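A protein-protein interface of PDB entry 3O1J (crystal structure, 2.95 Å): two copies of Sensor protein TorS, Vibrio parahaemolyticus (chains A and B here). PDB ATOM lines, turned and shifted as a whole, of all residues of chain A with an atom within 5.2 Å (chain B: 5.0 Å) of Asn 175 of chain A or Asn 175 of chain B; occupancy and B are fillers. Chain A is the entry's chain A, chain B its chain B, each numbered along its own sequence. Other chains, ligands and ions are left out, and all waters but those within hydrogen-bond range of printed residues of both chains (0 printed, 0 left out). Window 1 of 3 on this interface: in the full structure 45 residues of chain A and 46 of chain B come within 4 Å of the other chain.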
ATOM      1  N   PHE A 171      13.439 -22.601  18.072  1.00  0.00           N
ATOM      2  CA  PHE A 171      12.602 -22.311  19.219  1.00  0.00           C
ATOM      3  C   PHE A 171      12.887 -23.330  20.315  1.00  0.00           C
ATOM      4  O   PHE A 171      12.934 -22.983  21.494  1.00  0.00           O
ATOM      5  CB  PHE A 171      11.127 -22.358  18.807  1.00  0.00           C
ATOM      6  CG  PHE A 171      10.177 -21.939  19.891  1.00  0.00           C
ATOM      7  CD1 PHE A 171      10.138 -20.621  20.329  1.00  0.00           C
ATOM      8  CD2 PHE A 171       9.326 -22.867  20.484  1.00  0.00           C
ATOM      9  CE1 PHE A 171       9.264 -20.227  21.346  1.00  0.00           C
ATOM     10  CE2 PHE A 171       8.446 -22.487  21.503  1.00  0.00           C
ATOM     11  CZ  PHE A 171       8.416 -21.164  21.935  1.00  0.00           C
ATOM     12  N   LYS A 172      13.085 -24.587  19.921  1.00  0.00           N
ATOM     13  CA  LYS A 172      13.364 -25.644  20.886  1.00  0.00           C
ATOM     14  C   LYS A 172      14.635 -25.292  21.628  1.00  0.00           C
ATOM     15  O   LYS A 172      14.651 -25.222  22.859  1.00  0.00           O
ATOM     16  CB  LYS A 172      13.535 -26.997  20.184  1.00  0.00           C
ATOM     17  CG  LYS A 172      13.840 -28.174  21.125  1.00  0.00           C
ATOM     18  CD  LYS A 172      12.998 -28.117  22.423  1.00  0.00           C
ATOM     19  CE  LYS A 172      12.993 -29.444  23.216  1.00  0.00           C
ATOM     20  NZ  LYS A 172      12.013 -30.494  22.727  1.00  0.00           N
ATOM     21  N   MET A 173      15.692 -25.064  20.852  1.00  0.00           N
ATOM     22  CA  MET A 173      17.008 -24.705  21.358  1.00  0.00           C
ATOM     23  C   MET A 173      16.969 -23.539  22.336  1.00  0.00           C
ATOM     24  O   MET A 173      17.744 -23.506  23.287  1.00  0.00           O
ATOM     25  CB  MET A 173      17.914 -24.378  20.180  1.00  0.00           C
ATOM     26  CG  MET A 173      19.280 -23.854  20.559  1.00  0.00           C
ATOM     27  SD  MET A 173      20.402 -24.031  19.155  1.00  0.00           S
ATOM     28  CE  MET A 173      20.306 -25.870  18.895  1.00  0.00           C
ATOM     29  N   LEU A 174      16.075 -22.580  22.107  1.00  0.00           N
ATOM     30  CA  LEU A 174      15.959 -21.444  23.010  1.00  0.00           C
ATOM     31  C   LEU A 174      15.420 -21.903  24.357  1.00  0.00           C
ATOM     32  O   LEU A 174      15.951 -21.524  25.399  1.00  0.00           O
ATOM     33  CB  LEU A 174      15.034 -20.379  22.440  1.00  0.00           C
ATOM     34  CG  LEU A 174      14.783 -19.213  23.401  1.00  0.00           C
ATOM     35  CD1 LEU A 174      16.094 -18.544  23.772  1.00  0.00           C
ATOM     36  CD2 LEU A 174      13.854 -18.219  22.752  1.00  0.00           C
ATOM     37  N   ASN A 175      14.369 -22.721  24.337  1.00  0.00           N
ATOM     38  CA  ASN A 175      13.781 -23.241  25.569  1.00  0.00           C
ATOM     39  C   ASN A 175      14.776 -24.067  26.373  1.00  0.00           C
ATOM     40  O   ASN A 175      14.737 -24.056  27.600  1.00  0.00           O
ATOM     41  CB  ASN A 175      12.565 -24.100  25.260  1.00  0.00           C
ATOM     42  CG  ASN A 175      11.414 -23.294  24.712  1.00  0.00           C
ATOM     43  OD1 ASN A 175      10.358 -23.851  24.389  1.00  0.00           O
ATOM     44  ND2 ASN A 175      11.600 -21.971  24.604  1.00  0.00           N
ATOM     45  N   GLN A 176      15.660 -24.795  25.692  1.00  0.00           N
ATOM     46  CA  GLN A 176      16.649 -25.596  26.398  1.00  0.00           C
ATOM     47  C   GLN A 176      17.505 -24.647  27.221  1.00  0.00           C
ATOM     48  O   GLN A 176      17.759 -24.893  28.392  1.00  0.00           O
ATOM     49  CB  GLN A 176      17.535 -26.368  25.423  1.00  0.00           C
ATOM     50  CG  GLN A 176      16.793 -26.916  24.234  1.00  0.00           C
ATOM     51  CD  GLN A 176      17.556 -28.007  23.504  1.00  0.00           C
ATOM     52  OE1 GLN A 176      17.619 -29.139  23.967  1.00  0.00           O
ATOM     53  NE2 GLN A 176      18.144 -27.667  22.361  1.00  0.00           N
ATOM     54  N   ILE A 177      17.928 -23.547  26.613  1.00  0.00           N
ATOM     55  CA  ILE A 177      18.758 -22.584  27.322  1.00  0.00           C
ATOM     56  C   ILE A 177      18.006 -21.925  28.481  1.00  0.00           C
ATOM     57  O   ILE A 177      18.560 -21.750  29.568  1.00  0.00           O
ATOM     58  CB  ILE A 177      19.315 -21.531  26.340  1.00  0.00           C
ATOM     59  CG1 ILE A 177      20.271 -22.225  25.376  1.00  0.00           C
ATOM     60  CG2 ILE A 177      20.054 -20.428  27.075  1.00  0.00           C
ATOM     61  CD1 ILE A 177      20.955 -21.291  24.433  1.00  0.00           C
ATOM     62  N   GLU A 178      16.743 -21.577  28.270  1.00  0.00           N
ATOM     63  CA  GLU A 178      15.964 -20.962  29.342  1.00  0.00           C
ATOM     64  C   GLU A 178      15.904 -21.893  30.561  1.00  0.00           C
ATOM     65  O   GLU A 178      16.075 -21.467  31.706  1.00  0.00           O
ATOM     66  CB  GLU A 178      14.539 -20.668  28.878  1.00  0.00           C
ATOM     67  CG  GLU A 178      14.403 -19.654  27.746  1.00  0.00           C
ATOM     68  CD  GLU A 178      12.928 -19.400  27.388  1.00  0.00           C
ATOM     69  OE1 GLU A 178      12.661 -18.691  26.382  1.00  0.00           O
ATOM     70  OE2 GLU A 178      12.038 -19.910  28.125  1.00  0.00           O
ATOM     71  N   GLU A 179      15.651 -23.170  30.315  1.00  0.00           N
ATOM     72  CA  GLU A 179      15.570 -24.124  31.401  1.00  0.00           C
ATOM     73  C   GLU A 179      16.942 -24.392  32.003  1.00  0.00           C
ATOM     74  O   GLU A 179      17.060 -24.704  33.191  1.00  0.00           O
ATOM     75  CB  GLU A 179      14.953 -25.436  30.909  1.00  0.00           C
ATOM     76  CG  GLU A 179      15.350 -26.642  31.747  1.00  0.00           C
ATOM     77  CD  GLU A 179      14.546 -27.894  31.442  1.00  0.00           C
ATOM     78  OE1 GLU A 179      14.328 -28.196  30.250  1.00  0.00           O
ATOM     79  OE2 GLU A 179      14.143 -28.587  32.403  1.00  0.00           O
ATOM     80  N   ALA A 180      17.979 -24.246  31.188  1.00  0.00           N
ATOM     81  CA  ALA A 180      19.344 -24.524  31.616  1.00  0.00           C
ATOM     82  C   ALA A 180      19.841 -23.779  32.836  1.00  0.00           C
ATOM     83  O   ALA A 180      20.385 -24.386  33.755  1.00  0.00           O
ATOM     84  CB  ALA A 180      20.298 -24.299  30.459  1.00  0.00           C
ATOM     85  N   PHE B 171       3.652 -26.849  21.290  1.00  0.00           N
ATOM     86  CA  PHE B 171       4.985 -27.382  21.435  1.00  0.00           C
ATOM     87  C   PHE B 171       5.579 -26.751  22.670  1.00  0.00           C
ATOM     88  O   PHE B 171       6.267 -27.413  23.437  1.00  0.00           O
ATOM     89  CB  PHE B 171       5.837 -27.016  20.230  1.00  0.00           C
ATOM     90  CG  PHE B 171       7.176 -27.679  20.224  1.00  0.00           C
ATOM     91  CD1 PHE B 171       7.298 -29.019  19.857  1.00  0.00           C
ATOM     92  CD2 PHE B 171       8.315 -26.977  20.596  1.00  0.00           C
ATOM     93  CE1 PHE B 171       8.536 -29.651  19.858  1.00  0.00           C
ATOM     94  CE2 PHE B 171       9.566 -27.596  20.603  1.00  0.00           C
ATOM     95  CZ  PHE B 171       9.678 -28.939  20.232  1.00  0.00           C
ATOM     96  N   LYS B 172       5.310 -25.460  22.851  1.00  0.00           N
ATOM     97  CA  LYS B 172       5.832 -24.734  23.998  1.00  0.00           C
ATOM     98  C   LYS B 172       5.331 -25.382  25.275  1.00  0.00           C
ATOM     99  O   LYS B 172       6.107 -25.718  26.175  1.00  0.00           O
ATOM    100  CB  LYS B 172       5.395 -23.265  23.957  1.00  0.00           C
ATOM    101  CG  LYS B 172       5.948 -22.424  25.118  1.00  0.00           C
ATOM    102  CD  LYS B 172       7.346 -22.943  25.558  1.00  0.00           C
ATOM    103  CE  LYS B 172       8.131 -21.959  26.443  1.00  0.00           C
ATOM    104  NZ  LYS B 172       8.777 -20.848  25.645  1.00  0.00           N
ATOM    105  N   MET B 173       4.019 -25.558  25.326  1.00  0.00           N
ATOM    106  CA  MET B 173       3.334 -26.164  26.451  1.00  0.00           C
ATOM    107  C   MET B 173       3.936 -27.510  26.840  1.00  0.00           C
ATOM    108  O   MET B 173       4.080 -27.819  28.024  1.00  0.00           O
ATOM    109  CB  MET B 173       1.871 -26.325  26.075  1.00  0.00           C
ATOM    110  CG  MET B 173       0.995 -26.901  27.153  1.00  0.00           C
ATOM    111  SD  MET B 173      -0.700 -26.431  26.797  1.00  0.00           S
ATOM    112  CE  MET B 173      -0.572 -24.618  26.958  1.00  0.00           C
ATOM    113  N   LEU B 174       4.289 -28.306  25.835  1.00  0.00           N
ATOM    114  CA  LEU B 174       4.873 -29.621  26.064  1.00  0.00           C
ATOM    115  C   LEU B 174       6.230 -29.535  26.753  1.00  0.00           C
ATOM    116  O   LEU B 174       6.558 -30.372  27.595  1.00  0.00           O
ATOM    117  CB  LEU B 174       5.018 -30.380  24.746  1.00  0.00           C
ATOM    118  CG  LEU B 174       5.652 -31.763  24.905  1.00  0.00           C
ATOM    119  CD1 LEU B 174       4.896 -32.525  25.975  1.00  0.00           C
ATOM    120  CD2 LEU B 174       5.628 -32.525  23.596  1.00  0.00           C
ATOM    121  N   ASN B 175       7.026 -28.530  26.394  1.00  0.00           N
ATOM    122  CA  ASN B 175       8.332 -28.362  27.013  1.00  0.00           C
ATOM    123  C   ASN B 175       8.181 -27.882  28.438  1.00  0.00           C
ATOM    124  O   ASN B 175       8.973 -28.255  29.301  1.00  0.00           O
ATOM    125  CB  ASN B 175       9.191 -27.373  26.235  1.00  0.00           C
ATOM    126  CG  ASN B 175       9.769 -27.975  24.970  1.00  0.00           C
ATOM    127  OD1 ASN B 175      10.563 -27.330  24.273  1.00  0.00           O
ATOM    128  ND2 ASN B 175       9.376 -29.217  24.659  1.00  0.00           N
ATOM    129  N   GLN B 176       7.176 -27.050  28.695  1.00  0.00           N
ATOM    130  CA  GLN B 176       6.969 -26.576  30.053  1.00  0.00           C
ATOM    131  C   GLN B 176       6.748 -27.809  30.925  1.00  0.00           C
ATOM    132  O   GLN B 176       7.248 -27.896  32.033  1.00  0.00           O
ATOM    133  CB  GLN B 176       5.749 -25.661  30.135  1.00  0.00           C
ATOM    134  CG  GLN B 176       5.636 -24.697  28.986  1.00  0.00           C
ATOM    135  CD  GLN B 176       4.674 -23.561  29.264  1.00  0.00           C
ATOM    136  OE1 GLN B 176       5.050 -22.568  29.874  1.00  0.00           O
ATOM    137  NE2 GLN B 176       3.423 -23.704  28.828  1.00  0.00           N
ATOM    138  N   ILE B 177       6.022 -28.782  30.402  1.00  0.00           N
ATOM    139  CA  ILE B 177       5.755 -29.986  31.161  1.00  0.00           C
ATOM    140  C   ILE B 177       6.981 -30.882  31.318  1.00  0.00           C
ATOM    141  O   ILE B 177       7.166 -31.496  32.361  1.00  0.00           O
ATOM    142  CB  ILE B 177       4.587 -30.749  30.524  1.00  0.00           C
ATOM    143  CG1 ILE B 177       3.314 -29.924  30.702  1.00  0.00           C
ATOM    144  CG2 ILE B 177       4.441 -32.127  31.132  1.00  0.00           C
ATOM    145  CD1 ILE B 177       2.094 -30.563  30.145  1.00  0.00           C
ATOM    146  N   GLU B 178       7.826 -30.956  30.297  1.00  0.00           N
ATOM    147  CA  GLU B 178       9.027 -31.786  30.393  1.00  0.00           C
ATOM    148  C   GLU B 178       9.980 -31.214  31.453  1.00  0.00           C
ATOM    149  O   GLU B 178      10.632 -31.954  32.192  1.00  0.00           O
ATOM    150  CB  GLU B 178       9.760 -31.840  29.048  1.00  0.00           C
ATOM    151  CG  GLU B 178       8.967 -32.417  27.874  1.00  0.00           C
ATOM    152  CD  GLU B 178       9.711 -32.275  26.529  1.00  0.00           C
ATOM    153  OE1 GLU B 178       9.107 -32.613  25.475  1.00  0.00           O
ATOM    154  OE2 GLU B 178      10.893 -31.826  26.524  1.00  0.00           O
ATOM    155  N   GLU B 179      10.070 -29.890  31.516  1.00  0.00           N
ATOM    156  CA  GLU B 179      10.942 -29.247  32.486  1.00  0.00           C
ATOM    157  C   GLU B 179      10.321 -29.316  33.858  1.00  0.00           C
ATOM    158  O   GLU B 179      11.026 -29.277  34.864  1.00  0.00           O
ATOM    159  CB  GLU B 179      11.172 -27.779  32.133  1.00  0.00           C
ATOM    160  CG  GLU B 179      11.629 -26.943  33.322  1.00  0.00           C
ATOM    161  CD  GLU B 179      12.032 -25.524  32.950  1.00  0.00           C
ATOM    162  OE1 GLU B 179      11.531 -25.004  31.931  1.00  0.00           O
ATOM    163  OE2 GLU B 179      12.842 -24.921  33.687  1.00  0.00           O
ATOM    164  N   ALA B 180       8.997 -29.432  33.877  1.00  0.00           N
ATOM    165  CA  ALA B 180       8.207 -29.467  35.103  1.00  0.00           C
ATOM    166  C   ALA B 180       8.624 -30.465  36.169  1.00  0.00           C
ATOM    167  O   ALA B 180       8.758 -30.086  37.328  1.00  0.00           O
ATOM    168  CB  ALA B 180       6.736 -29.662  34.763  1.00  0.00           C
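Among the printed residues, 6 pairs touch across the chains.
Among the printed residues, no Asp or Glu carboxylate lies within 4 Å of a Lys or Arg side-chain nitrogen of the other chain.
The side-chain amide nitrogen of Asn 175 of chain A sits close to the side-chain amino group of Lys 172 of chain B (3.2 Å).
The side-chain amide oxygen (OD1) of Asn 175 of chain A sits close to the side-chain amide oxygen (OD1) of Asn 175 of chain B (3.5 Å).
Phe 171 of chain A touches Lys 172 of chain B, and with the chains exchanged Lys 172 of chain A touches Phe 171 of chain B.
Lys 172 of chain A touches Asn 175 of chain B, and with the chains exchanged Asn 175 of chain A touches Lys 172 of chain B.
Asn 175 of chain B touches its own counterpart, Asn 175 of chain A.
Glu 179 of chain A touches its own counterpart, Glu 179 of chain B.
Asn 175 of chain A touches two residues of chain B.
Printed residues of chain A within 4 Å of Asn 175 of chain B: Lys 172 and Asn 175.
Of the printed residues of chain B, Phe 171 of chain A touches Lys 172.
Printed residues of chain A within 4 Å of Glu 179 of chain B: Glu 179 (3.1 Å).
Among the printed residues, merely in contact across the chains: Phe 171 of chain A with Lys 172 of chain B, Lys 172 of chain A with Phe 171 of chain B, Lys 172 of chain A with Asn 175 of chain B and Glu 179 of chain A with Glu 179 of chain B.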
